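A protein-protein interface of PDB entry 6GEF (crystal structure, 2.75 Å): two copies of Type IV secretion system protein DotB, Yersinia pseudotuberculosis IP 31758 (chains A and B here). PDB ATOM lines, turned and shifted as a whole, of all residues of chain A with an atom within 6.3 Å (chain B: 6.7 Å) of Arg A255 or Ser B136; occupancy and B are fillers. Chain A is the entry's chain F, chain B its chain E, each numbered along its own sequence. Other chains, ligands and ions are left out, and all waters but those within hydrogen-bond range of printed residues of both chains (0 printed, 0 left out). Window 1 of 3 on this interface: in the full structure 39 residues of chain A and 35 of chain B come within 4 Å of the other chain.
OD2 of Asp B55 is in salt-bridge range of NZ of Lys B67 (3.9 Å). OD1 of Asn B109 lies within hydrogen-bond range of ND2 of Asn B134 (2.9 Å). The side-chain amide oxygen (OD1) of Asn B134 sits at hydrogen-bond distance from the side-chain hydroxyl (OG) of Ser B136. The backbone NH (N) of Asn B134 lies within hydrogen-bond range of the backbone carbonyl oxygen (O) of Val B149, at 2.9 Å. O of His A211 is in hydrogen-bond range of N of Asn A258. The guanidinium group (NE) of Arg A254 is in salt-bridge range of the side-chain carboxylate (OE2) of Glu A251 (3.7 Å).
No position is printed for both chains. Of the 22 pairs that touch across the chains among the printed residues, none has its exchanged pair printed and touching as well.
Ala A252 touches none of the printed residues of chain B. Of the printed residues of chain B, Arg A254 touches Asn B109 (3.1 Å), Val B149 (3.9 Å) and Arg B151 (2.4 Å). Arg A255 touches just these residues of chain B: Asn B134 (3.4 Å), Ser B136 (3.5 Å), Val B138 (3.5 Å), Glu B147 (2.8 Å) and Val B149 (3.7 Å). Of the printed residues of chain A, Asp B55 touches Thr A256 (2.3 Å). Of the printed residues of chain A, Ile B57 touches His A211. Printed residues of chain A within 4 Å of Asn B109: Glu A251 and Arg A254. Of chain A, only Phe A242 (3.7 Å) and Arg A255 (3.5 Å) come within 4 Å of Ser B136. Thr B145 touches none of the printed residues of chain A. Of the printed residues of chain A, Val B149 touches Arg A254 (3.9 Å), Arg A255 (3.7 Å) and Thr A256 (3.5 Å). The nearest residue of chain B that does not touch Arg A255 is Arg B151 (4.3 Å). The nearest printed residue of chain A that does not touch Asp B55 is Arg A255 (6.1 Å).
His A211 touches Ile B57. Ala A234 touches Glu B147. CG1 of Val B138 touches O of Gln A235, 3.2 Å away. Phe A242 touches Ser B136. Pro B137 touches Phe A242. Arg A254 touches Asn B109 (CD to OD1, 3.1 Å). Arg A255 touches Asn B134. Arg A255 touches Val B138. Val B149 touches Arg A255. Val B149 touches Thr A256 (CG1 to CG2, 3.5 Å).
Of the 16 printed residues of chain A, 10 touch a printed residue of chain B. Printed residues of chain A that touch a printed residue of chain B: His A211, Ala A234, Gln A235, Ser A236, Phe A242, Glu A251, Arg A254, Arg A255, Thr A256 and Asn A258. Hydrophobic or aromatic side chains of chain A that line the printed part of chain B: His A211, Ala A234 and Phe A242. Of the 17 printed residues of chain B, 11 touch a printed residue of chain A. Printed residues of chain B that touch a printed residue of chain A: Asp B55, Ile B57, Lys B67, Asn B109, Asn B134, Ser B136, Pro B137, Val B138, Glu B147, Val B149 and Arg B151. Hydrophobic or aromatic side chains of chain B that line the printed part of chain A: Ile B57, Pro B137, Val B138 and Val B149. Among the printed residues, 22 pairs touch across the chains. Among the printed residues, Asp or Glu carboxylates within 4 Å of a Lys or Arg side-chain nitrogen of the other chain: Arg A255 with Glu B147.
NZ of Lys B67 lies within hydrogen-bond range of OG1 of Thr A256. NZ of Lys B67 lies close to OD1 of Asn A258. ND2 of Asn B109 lies within hydrogen-bond range of OE2 of Glu A251 (3.1 Å). OE1 of Glu A251 is in hydrogen-bond range of ND2 of Asn B134, at 2.8 Å. The side-chain hydroxyl of Ser A236 sits at hydrogen-bond distance from the backbone carbonyl oxygen of Pro B137 (3.0 Å). OE1 of Glu B147 lies close to NE2 of His A211 (3.0 Å). The guanidinium group (NH2) of Arg A255 lies within salt-bridge range of the side-chain carboxylate (OE2) of Glu B147 (2.8 Å). The backbone carbonyl oxygen (O) of Arg A254 lies close to the guanidinium group (NH1) of Arg B151, at 2.4 Å. The side-chain carboxylate of Asp B55 lies close to the side-chain hydroxyl of Thr A256.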
ATOM      1  N   HIS A 211      19.977   3.620 -10.191  1.00  0.00           N
ATOM      2  CA  HIS A 211      18.839   3.016  -9.507  1.00  0.00           C
ATOM      3  C   HIS A 211      17.911   2.380 -10.518  1.00  0.00           C
ATOM      4  O   HIS A 211      17.399   3.050 -11.406  1.00  0.00           O
ATOM      5  CB  HIS A 211      18.091   4.065  -8.691  1.00  0.00           C
ATOM      6  CG  HIS A 211      17.429   3.510  -7.465  1.00  0.00           C
ATOM      7  ND1 HIS A 211      17.441   2.161  -7.134  1.00  0.00           N
ATOM      8  CD2 HIS A 211      16.696   4.112  -6.492  1.00  0.00           C
ATOM      9  CE1 HIS A 211      16.772   1.972  -6.027  1.00  0.00           C
ATOM     10  NE2 HIS A 211      16.314   3.135  -5.609  1.00  0.00           N
ATOM     11  N   LEU A 213      14.445   0.277 -10.723  1.00  0.00           N
ATOM     12  CA  LEU A 213      13.222  -0.208 -10.120  1.00  0.00           C
ATOM     13  C   LEU A 213      12.479  -1.073 -11.088  1.00  0.00           C
ATOM     14  O   LEU A 213      12.407  -0.763 -12.275  1.00  0.00           O
ATOM     15  CB  LEU A 213      12.334   0.985  -9.667  1.00  0.00           C
ATOM     16  CG  LEU A 213      13.027   2.129  -8.973  1.00  0.00           C
ATOM     17  CD1 LEU A 213      11.990   3.127  -8.491  1.00  0.00           C
ATOM     18  CD2 LEU A 213      13.857   1.599  -7.794  1.00  0.00           C
ATOM     19  N   HIS A 215       8.538  -2.793 -11.158  1.00  0.00           N
ATOM     20  CA  HIS A 215       7.230  -3.115 -10.625  1.00  0.00           C
ATOM     21  C   HIS A 215       6.710  -4.359 -11.331  1.00  0.00           C
ATOM     22  O   HIS A 215       6.317  -4.319 -12.489  1.00  0.00           O
ATOM     23  CB  HIS A 215       6.277  -1.942 -10.827  1.00  0.00           C
ATOM     24  CG  HIS A 215       6.843  -0.606 -10.449  1.00  0.00           C
ATOM     25  ND1 HIS A 215       7.776  -0.458  -9.462  1.00  0.00           N
ATOM     26  CD2 HIS A 215       6.592   0.629 -10.912  1.00  0.00           C
ATOM     27  CE1 HIS A 215       8.092   0.819  -9.337  1.00  0.00           C
ATOM     28  NE2 HIS A 215       7.392   1.500 -10.214  1.00  0.00           N
ATOM     29  N   ALA A 234      15.914  -2.564  -7.225  1.00  0.00           N
ATOM     30  CA  ALA A 234      14.891  -2.727  -6.192  1.00  0.00           C
ATOM     31  C   ALA A 234      13.618  -3.183  -6.873  1.00  0.00           C
ATOM     32  O   ALA A 234      13.078  -2.479  -7.736  1.00  0.00           O
ATOM     33  CB  ALA A 234      14.637  -1.446  -5.407  1.00  0.00           C
ATOM     34  N   GLN A 235      13.107  -4.350  -6.526  1.00  0.00           N
ATOM     35  CA  GLN A 235      11.895  -4.905  -7.065  1.00  0.00           C
ATOM     36  C   GLN A 235      10.758  -4.787  -6.083  1.00  0.00           C
ATOM     37  O   GLN A 235      10.960  -4.803  -4.856  1.00  0.00           O
ATOM     38  CB  GLN A 235      12.107  -6.391  -7.403  1.00  0.00           C
ATOM     39  CG  GLN A 235      13.255  -6.669  -8.360  1.00  0.00           C
ATOM     40  CD  GLN A 235      13.545  -8.141  -8.475  1.00  0.00           C
ATOM     41  OE1 GLN A 235      14.526  -8.642  -7.899  1.00  0.00           O
ATOM     42  NE2 GLN A 235      12.734  -8.850  -9.225  1.00  0.00           N
ATOM     43  N   SER A 236       9.545  -4.652  -6.614  1.00  0.00           N
ATOM     44  CA  SER A 236       8.338  -4.469  -5.802  1.00  0.00           C
ATOM     45  C   SER A 236       7.231  -5.317  -6.373  1.00  0.00           C
ATOM     46  O   SER A 236       6.978  -5.275  -7.573  1.00  0.00           O
ATOM     47  CB  SER A 236       7.929  -3.002  -5.774  1.00  0.00           C
ATOM     48  OG  SER A 236       8.994  -2.208  -5.220  1.00  0.00           O
ATOM     49  N   PHE A 242       3.062  -2.723  -3.249  1.00  0.00           N
ATOM     50  CA  PHE A 242       2.302  -1.563  -3.693  1.00  0.00           C
ATOM     51  C   PHE A 242       0.912  -1.998  -4.136  1.00  0.00           C
ATOM     52  O   PHE A 242       0.733  -3.060  -4.727  1.00  0.00           O
ATOM     53  CB  PHE A 242       2.989  -0.883  -4.859  1.00  0.00           C
ATOM     54  CG  PHE A 242       4.133   0.012  -4.463  1.00  0.00           C
ATOM     55  CD1 PHE A 242       3.909   1.109  -3.669  1.00  0.00           C
ATOM     56  CD2 PHE A 242       5.403  -0.231  -4.918  1.00  0.00           C
ATOM     57  CE1 PHE A 242       4.957   1.946  -3.310  1.00  0.00           C
ATOM     58  CE2 PHE A 242       6.454   0.598  -4.574  1.00  0.00           C
ATOM     59  CZ  PHE A 242       6.228   1.687  -3.762  1.00  0.00           C
ATOM     60  N   ALA A 248       2.587   2.617  -7.450  1.00  0.00           N
ATOM     61  CA  ALA A 248       4.007   2.326  -7.627  1.00  0.00           C
ATOM     62  C   ALA A 248       4.665   3.372  -8.520  1.00  0.00           C
ATOM     63  O   ALA A 248       5.779   3.803  -8.225  1.00  0.00           O
ATOM     64  CB  ALA A 248       4.179   0.940  -8.241  1.00  0.00           C
ATOM     65  N   GLU A 251       4.932   6.792  -6.805  1.00  0.00           N
ATOM     66  CA  GLU A 251       6.033   6.739  -5.831  1.00  0.00           C
ATOM     67  C   GLU A 251       7.409   6.660  -6.520  1.00  0.00           C
ATOM     68  O   GLU A 251       8.381   7.112  -5.979  1.00  0.00           O
ATOM     69  CB  GLU A 251       5.850   5.554  -4.887  1.00  0.00           C
ATOM     70  CG  GLU A 251       4.765   5.752  -3.856  1.00  0.00           C
ATOM     71  CD  GLU A 251       5.129   6.770  -2.800  1.00  0.00           C
ATOM     72  OE1 GLU A 251       5.744   6.302  -1.803  1.00  0.00           O
ATOM     73  OE2 GLU A 251       4.759   7.961  -2.921  1.00  0.00           O
ATOM     74  N   ALA A 252       7.447   6.118  -7.727  1.00  0.00           N
ATOM     75  CA  ALA A 252       8.731   5.833  -8.364  1.00  0.00           C
ATOM     76  C   ALA A 252       9.494   7.124  -8.642  1.00  0.00           C
ATOM     77  O   ALA A 252      10.730   7.175  -8.461  1.00  0.00           O
ATOM     78  CB  ALA A 252       8.526   5.040  -9.645  1.00  0.00           C
ATOM     79  N   LEU A 253       8.815   8.163  -9.092  1.00  0.00           N
ATOM     80  CA  LEU A 253       9.472   9.436  -9.350  1.00  0.00           C
ATOM     81  C   LEU A 253      10.015  10.081  -8.124  1.00  0.00           C
ATOM     82  O   LEU A 253      10.752  11.072  -8.211  1.00  0.00           O
ATOM     83  CB  LEU A 253       8.532  10.373 -10.148  1.00  0.00           C
ATOM     84  CG  LEU A 253       7.028  10.273  -9.811  1.00  0.00           C
ATOM     85  CD1 LEU A 253       6.582  11.339  -8.846  1.00  0.00           C
ATOM     86  CD2 LEU A 253       6.269  10.284 -11.119  1.00  0.00           C
ATOM     87  N   ARG A 254       9.622   9.637  -6.937  1.00  0.00           N
ATOM     88  CA  ARG A 254      10.236  10.071  -5.676  1.00  0.00           C
ATOM     89  C   ARG A 254      11.463   9.285  -5.298  1.00  0.00           C
ATOM     90  O   ARG A 254      12.058   9.578  -4.275  1.00  0.00           O
ATOM     91  CB  ARG A 254       9.193  10.009  -4.554  1.00  0.00           C
ATOM     92  CG  ARG A 254       7.920  10.766  -4.877  1.00  0.00           C
ATOM     93  CD  ARG A 254       7.184  11.117  -3.611  1.00  0.00           C
ATOM     94  NE  ARG A 254       5.768  11.373  -3.859  1.00  0.00           N
ATOM     95  CZ  ARG A 254       5.098  12.393  -3.345  1.00  0.00           C
ATOM     96  NH1 ARG A 254       5.726  13.263  -2.552  1.00  0.00           N
ATOM     97  NH2 ARG A 254       3.801  12.540  -3.631  1.00  0.00           N
ATOM     98  N   ARG A 255      11.859   8.288  -6.092  1.00  0.00           N
ATOM     99  CA  ARG A 255      12.931   7.371  -5.734  1.00  0.00           C
ATOM    100  C   ARG A 255      14.120   7.447  -6.653  1.00  0.00           C
ATOM    101  O   ARG A 255      14.945   6.532  -6.704  1.00  0.00           O
ATOM    102  CB  ARG A 255      12.403   5.928  -5.665  1.00  0.00           C
ATOM    103  CG  ARG A 255      11.155   5.763  -4.799  1.00  0.00           C
ATOM    104  CD  ARG A 255      10.499   4.454  -4.995  1.00  0.00           C
ATOM    105  NE  ARG A 255      11.362   3.309  -4.654  1.00  0.00           N
ATOM    106  CZ  ARG A 255      11.102   2.055  -4.919  1.00  0.00           C
ATOM    107  NH1 ARG A 255      10.001   1.718  -5.504  1.00  0.00           N
ATOM    108  NH2 ARG A 255      11.963   1.122  -4.591  1.00  0.00           N
ATOM    109  N   THR A 256      14.235   8.544  -7.409  1.00  0.00           N
ATOM    110  CA  THR A 256      15.426   8.816  -8.213  1.00  0.00           C
ATOM    111  C   THR A 256      15.854   7.613  -9.042  1.00  0.00           C
ATOM    112  O   THR A 256      17.018   7.274  -9.064  1.00  0.00           O
ATOM    113  CB  THR A 256      16.572   9.237  -7.272  1.00  0.00           C
ATOM    114  OG1 THR A 256      17.677   9.727  -8.007  1.00  0.00           O
ATOM    115  CG2 THR A 256      17.032   8.019  -6.336  1.00  0.00           C
ATOM    116  N   PRO A 257      14.932   6.932  -9.705  1.00  0.00           N
ATOM    117  CA  PRO A 257      15.310   5.813 -10.556  1.00  0.00           C
ATOM    118  C   PRO A 257      16.094   6.252 -11.786  1.00  0.00           C
ATOM    119  O   PRO A 257      15.868   7.323 -12.341  1.00  0.00           O
ATOM    120  CB  PRO A 257      13.959   5.202 -10.984  1.00  0.00           C
ATOM    121  CG  PRO A 257      13.008   6.310 -10.899  1.00  0.00           C
ATOM    122  CD  PRO A 257      13.468   7.172  -9.767  1.00  0.00           C
ATOM    123  N   ASN A 258      17.034   5.407 -12.182  1.00  0.00           N
ATOM    124  CA  ASN A 258      17.620   5.444 -13.506  1.00  0.00           C
ATOM    125  C   ASN A 258      17.028   4.449 -14.483  1.00  0.00           C
ATOM    126  O   ASN A 258      17.362   4.456 -15.654  1.00  0.00           O
ATOM    127  CB  ASN A 258      19.149   5.260 -13.414  1.00  0.00           C
ATOM    128  CG  ASN A 258      19.792   6.106 -12.376  1.00  0.00           C
ATOM    129  OD1 ASN A 258      19.573   5.905 -11.185  1.00  0.00           O
ATOM    130  ND2 ASN A 258      20.597   7.043 -12.807  1.00  0.00           N
ATOM    131  N   ASP B  55      21.354  12.367  -4.086  1.00  0.00           N
ATOM    132  CA  ASP B  55      20.335  11.426  -3.660  1.00  0.00           C
ATOM    133  C   ASP B  55      20.968  10.310  -2.845  1.00  0.00           C
ATOM    134  O   ASP B  55      21.965   9.763  -3.258  1.00  0.00           O
ATOM    135  CB  ASP B  55      19.650  10.811  -4.885  1.00  0.00           C
ATOM    136  CG  ASP B  55      18.861  11.805  -5.690  1.00  0.00           C
ATOM    137  OD1 ASP B  55      18.361  12.799  -5.071  1.00  0.00           O
ATOM    138  OD2 ASP B  55      18.746  11.469  -6.937  1.00  0.00           O
ATOM    139  N   ILE B  57      20.349   6.648  -1.481  1.00  0.00           N
ATOM    140  CA  ILE B  57      19.644   5.368  -1.432  1.00  0.00           C
ATOM    141  C   ILE B  57      20.248   4.526  -0.310  1.00  0.00           C
ATOM    142  O   ILE B  57      21.454   4.319  -0.255  1.00  0.00           O
ATOM    143  CB  ILE B  57      19.752   4.621  -2.776  1.00  0.00           C
ATOM    144  CG1 ILE B  57      21.083   3.909  -2.891  1.00  0.00           C
ATOM    145  CG2 ILE B  57      19.419   5.507  -3.916  1.00  0.00           C
ATOM    146  CD1 ILE B  57      21.037   2.444  -2.398  1.00  0.00           C
ATOM    147  N   LYS B  67      24.056   9.532  -5.244  1.00  0.00           N
ATOM    148  CA  LYS B  67      24.393  10.029  -6.570  1.00  0.00           C
ATOM    149  C   LYS B  67      25.217  11.301  -6.425  1.00  0.00           C
ATOM    150  O   LYS B  67      24.706  12.398  -6.398  1.00  0.00           O
ATOM    151  CB  LYS B  67      23.110  10.273  -7.381  1.00  0.00           C
ATOM    152  CG  LYS B  67      22.217   9.068  -7.531  1.00  0.00           C
ATOM    153  CD  LYS B  67      21.590   8.942  -8.868  1.00  0.00           C
ATOM    154  CE  LYS B  67      20.693   7.748  -9.014  1.00  0.00           C
ATOM    155  NZ  LYS B  67      19.303   8.198  -8.990  1.00  0.00           N
ATOM    156  N   ALA B 103       4.648   0.126   6.577  1.00  0.00           N
ATOM    157  CA  ALA B 103       4.672   0.066   5.134  1.00  0.00           C
ATOM    158  C   ALA B 103       3.759  -0.995   4.583  1.00  0.00           C
ATOM    159  O   ALA B 103       3.891  -1.419   3.431  1.00  0.00           O
ATOM    160  CB  ALA B 103       6.124  -0.142   4.613  1.00  0.00           C
ATOM    161  N   ILE B 108       5.194   6.538   2.492  1.00  0.00           N
ATOM    162  CA  ILE B 108       5.991   7.203   3.511  1.00  0.00           C
ATOM    163  C   ILE B 108       6.853   8.224   2.839  1.00  0.00           C
ATOM    164  O   ILE B 108       7.924   7.888   2.300  1.00  0.00           O
ATOM    165  CB  ILE B 108       6.843   6.196   4.327  1.00  0.00           C
ATOM    166  CG1 ILE B 108       5.936   5.168   5.021  1.00  0.00           C
ATOM    167  CG2 ILE B 108       7.689   6.914   5.344  1.00  0.00           C
ATOM    168  CD1 ILE B 108       6.687   4.053   5.644  1.00  0.00           C
ATOM    169  N   ASN B 109       6.394   9.482   2.835  1.00  0.00           N
ATOM    170  CA  ASN B 109       7.174  10.614   2.335  1.00  0.00           C
ATOM    171  C   ASN B 109       7.294  11.631   3.440  1.00  0.00           C
ATOM    172  O   ASN B 109       6.306  12.192   3.850  1.00  0.00           O
ATOM    173  CB  ASN B 109       6.512  11.202   1.087  1.00  0.00           C
ATOM    174  CG  ASN B 109       6.498  10.242  -0.066  1.00  0.00           C
ATOM    175  OD1 ASN B 109       7.538  10.048  -0.714  1.00  0.00           O
ATOM    176  ND2 ASN B 109       5.354   9.671  -0.369  1.00  0.00           N
ATOM    177  N   ASN B 134      11.675   9.118   1.125  1.00  0.00           N
ATOM    178  CA  ASN B 134      10.618   8.213   0.717  1.00  0.00           C
ATOM    179  C   ASN B 134      11.018   6.782   1.059  1.00  0.00           C
ATOM    180  O   ASN B 134      12.109   6.344   0.704  1.00  0.00           O
ATOM    181  CB  ASN B 134      10.357   8.316  -0.778  1.00  0.00           C
ATOM    182  CG  ASN B 134       9.559   7.142  -1.322  1.00  0.00           C
ATOM    183  OD1 ASN B 134      10.125   6.082  -1.596  1.00  0.00           O
ATOM    184  ND2 ASN B 134       8.283   7.326  -1.498  1.00  0.00           N
ATOM    185  N   ILE B 135      10.125   6.073   1.758  1.00  0.00           N
ATOM    186  CA  ILE B 135      10.384   4.735   2.219  1.00  0.00           C
ATOM    187  C   ILE B 135       9.388   3.806   1.535  1.00  0.00           C
ATOM    188  O   ILE B 135       8.174   3.911   1.740  1.00  0.00           O
ATOM    189  CB  ILE B 135      10.258   4.623   3.753  1.00  0.00           C
ATOM    190  CG1 ILE B 135      11.185   5.632   4.448  1.00  0.00           C
ATOM    191  CG2 ILE B 135      10.521   3.186   4.206  1.00  0.00           C
ATOM    192  CD1 ILE B 135      11.432   5.347   5.896  1.00  0.00           C
ATOM    193  N   SER B 136       9.902   2.904   0.696  1.00  0.00           N
ATOM    194  CA  SER B 136       9.085   2.113  -0.182  1.00  0.00           C
ATOM    195  C   SER B 136       9.332   0.633   0.046  1.00  0.00           C
ATOM    196  O   SER B 136      10.461   0.229   0.318  1.00  0.00           O
ATOM    197  CB  SER B 136       9.442   2.459  -1.660  1.00  0.00           C
ATOM    198  OG  SER B 136       8.828   3.668  -2.069  1.00  0.00           O
ATOM    199  N   PRO B 137       8.275  -0.187  -0.081  1.00  0.00           N
ATOM    200  CA  PRO B 137       8.480  -1.632   0.092  1.00  0.00           C
ATOM    201  C   PRO B 137       9.273  -2.192  -1.082  1.00  0.00           C
ATOM    202  O   PRO B 137       8.899  -1.982  -2.259  1.00  0.00           O
ATOM    203  CB  PRO B 137       7.050  -2.167   0.161  1.00  0.00           C
ATOM    204  CG  PRO B 137       6.240  -1.132  -0.643  1.00  0.00           C
ATOM    205  CD  PRO B 137       6.869   0.169  -0.318  1.00  0.00           C
ATOM    206  N   VAL B 138      10.325  -2.922  -0.779  1.00  0.00           N
ATOM    207  CA  VAL B 138      11.108  -3.638  -1.780  1.00  0.00           C
ATOM    208  C   VAL B 138      11.231  -5.098  -1.346  1.00  0.00           C
ATOM    209  O   VAL B 138      11.134  -5.419  -0.176  1.00  0.00           O
ATOM    210  CB  VAL B 138      12.515  -3.009  -1.963  1.00  0.00           C
ATOM    211  CG1 VAL B 138      13.321  -3.718  -3.032  1.00  0.00           C
ATOM    212  CG2 VAL B 138      12.421  -1.553  -2.340  1.00  0.00           C
ATOM    213  N   THR B 145      11.376  -5.834   2.675  1.00  0.00           N
ATOM    214  CA  THR B 145      12.095  -4.804   3.412  1.00  0.00           C
ATOM    215  C   THR B 145      11.632  -3.418   2.961  1.00  0.00           C
ATOM    216  O   THR B 145      10.832  -3.278   2.048  1.00  0.00           O
ATOM    217  CB  THR B 145      13.612  -4.930   3.173  1.00  0.00           C
ATOM    218  OG1 THR B 145      13.956  -6.255   2.762  1.00  0.00           O
ATOM    219  CG2 THR B 145      14.374  -4.572   4.451  1.00  0.00           C
ATOM    220  N   ALA B 146      12.115  -2.415   3.635  1.00  0.00           N
ATOM    221  CA  ALA B 146      11.999  -1.029   3.209  1.00  0.00           C
ATOM    222  C   ALA B 146      13.287  -0.601   2.536  1.00  0.00           C
ATOM    223  O   ALA B 146      14.397  -0.975   2.955  1.00  0.00           O
ATOM    224  CB  ALA B 146      11.739  -0.095   4.395  1.00  0.00           C
ATOM    225  N   GLU B 147      13.133   0.160   1.438  1.00  0.00           N
ATOM    226  CA  GLU B 147      14.212   0.935   0.860  1.00  0.00           C
ATOM    227  C   GLU B 147      13.929   2.415   1.054  1.00  0.00           C
ATOM    228  O   GLU B 147      12.808   2.862   0.832  1.00  0.00           O
ATOM    229  CB  GLU B 147      14.392   0.610  -0.600  1.00  0.00           C
ATOM    230  CG  GLU B 147      15.608   1.244  -1.238  1.00  0.00           C
ATOM    231  CD  GLU B 147      15.528   1.236  -2.764  1.00  0.00           C
ATOM    232  OE1 GLU B 147      16.607   1.157  -3.365  1.00  0.00           O
ATOM    233  OE2 GLU B 147      14.440   1.394  -3.354  1.00  0.00           O
ATOM    234  N   ILE B 148      14.971   3.159   1.452  1.00  0.00           N
ATOM    235  CA  ILE B 148      14.861   4.581   1.717  1.00  0.00           C
ATOM    236  C   ILE B 148      15.585   5.349   0.584  1.00  0.00           C
ATOM    237  O   ILE B 148      16.668   4.970   0.165  1.00  0.00           O
ATOM    238  CB  ILE B 148      15.457   4.932   3.063  1.00  0.00           C
ATOM    239  CG1 ILE B 148      14.642   4.245   4.187  1.00  0.00           C
ATOM    240  CG2 ILE B 148      15.469   6.453   3.279  1.00  0.00           C
ATOM    241  CD1 ILE B 148      15.306   3.113   4.874  1.00  0.00           C
ATOM    242  N   VAL B 149      14.952   6.416   0.114  1.00  0.00           N
ATOM    243  CA  VAL B 149      15.545   7.343  -0.818  1.00  0.00           C
ATOM    244  C   VAL B 149      15.292   8.754  -0.294  1.00  0.00           C
ATOM    245  O   VAL B 149      14.174   9.227  -0.324  1.00  0.00           O
ATOM    246  CB  VAL B 149      14.965   7.160  -2.242  1.00  0.00           C
ATOM    247  CG1 VAL B 149      15.547   8.183  -3.200  1.00  0.00           C
ATOM    248  CG2 VAL B 149      15.327   5.783  -2.747  1.00  0.00           C
ATOM    249  N   ARG B 151      16.010  12.633  -1.242  1.00  0.00           N
ATOM    250  CA  ARG B 151      16.364  13.540  -2.327  1.00  0.00           C
ATOM    251  C   ARG B 151      16.790  14.871  -1.743  1.00  0.00           C
ATOM    252  O   ARG B 151      16.016  15.501  -1.006  1.00  0.00           O
ATOM    253  CB  ARG B 151      15.164  13.742  -3.251  1.00  0.00           C
ATOM    254  CG  ARG B 151      14.571  12.470  -3.818  1.00  0.00           C
ATOM    255  CD  ARG B 151      13.597  12.809  -4.936  1.00  0.00           C
ATOM    256  NE  ARG B 151      12.415  13.542  -4.494  1.00  0.00           N
ATOM    257  CZ  ARG B 151      11.359  12.994  -3.899  1.00  0.00           C
ATOM    258  NH1 ARG B 151      11.299  11.718  -3.628  1.00  0.00           N
ATOM    259  NH2 ARG B 151      10.329  13.744  -3.523  1.00  0.00           N
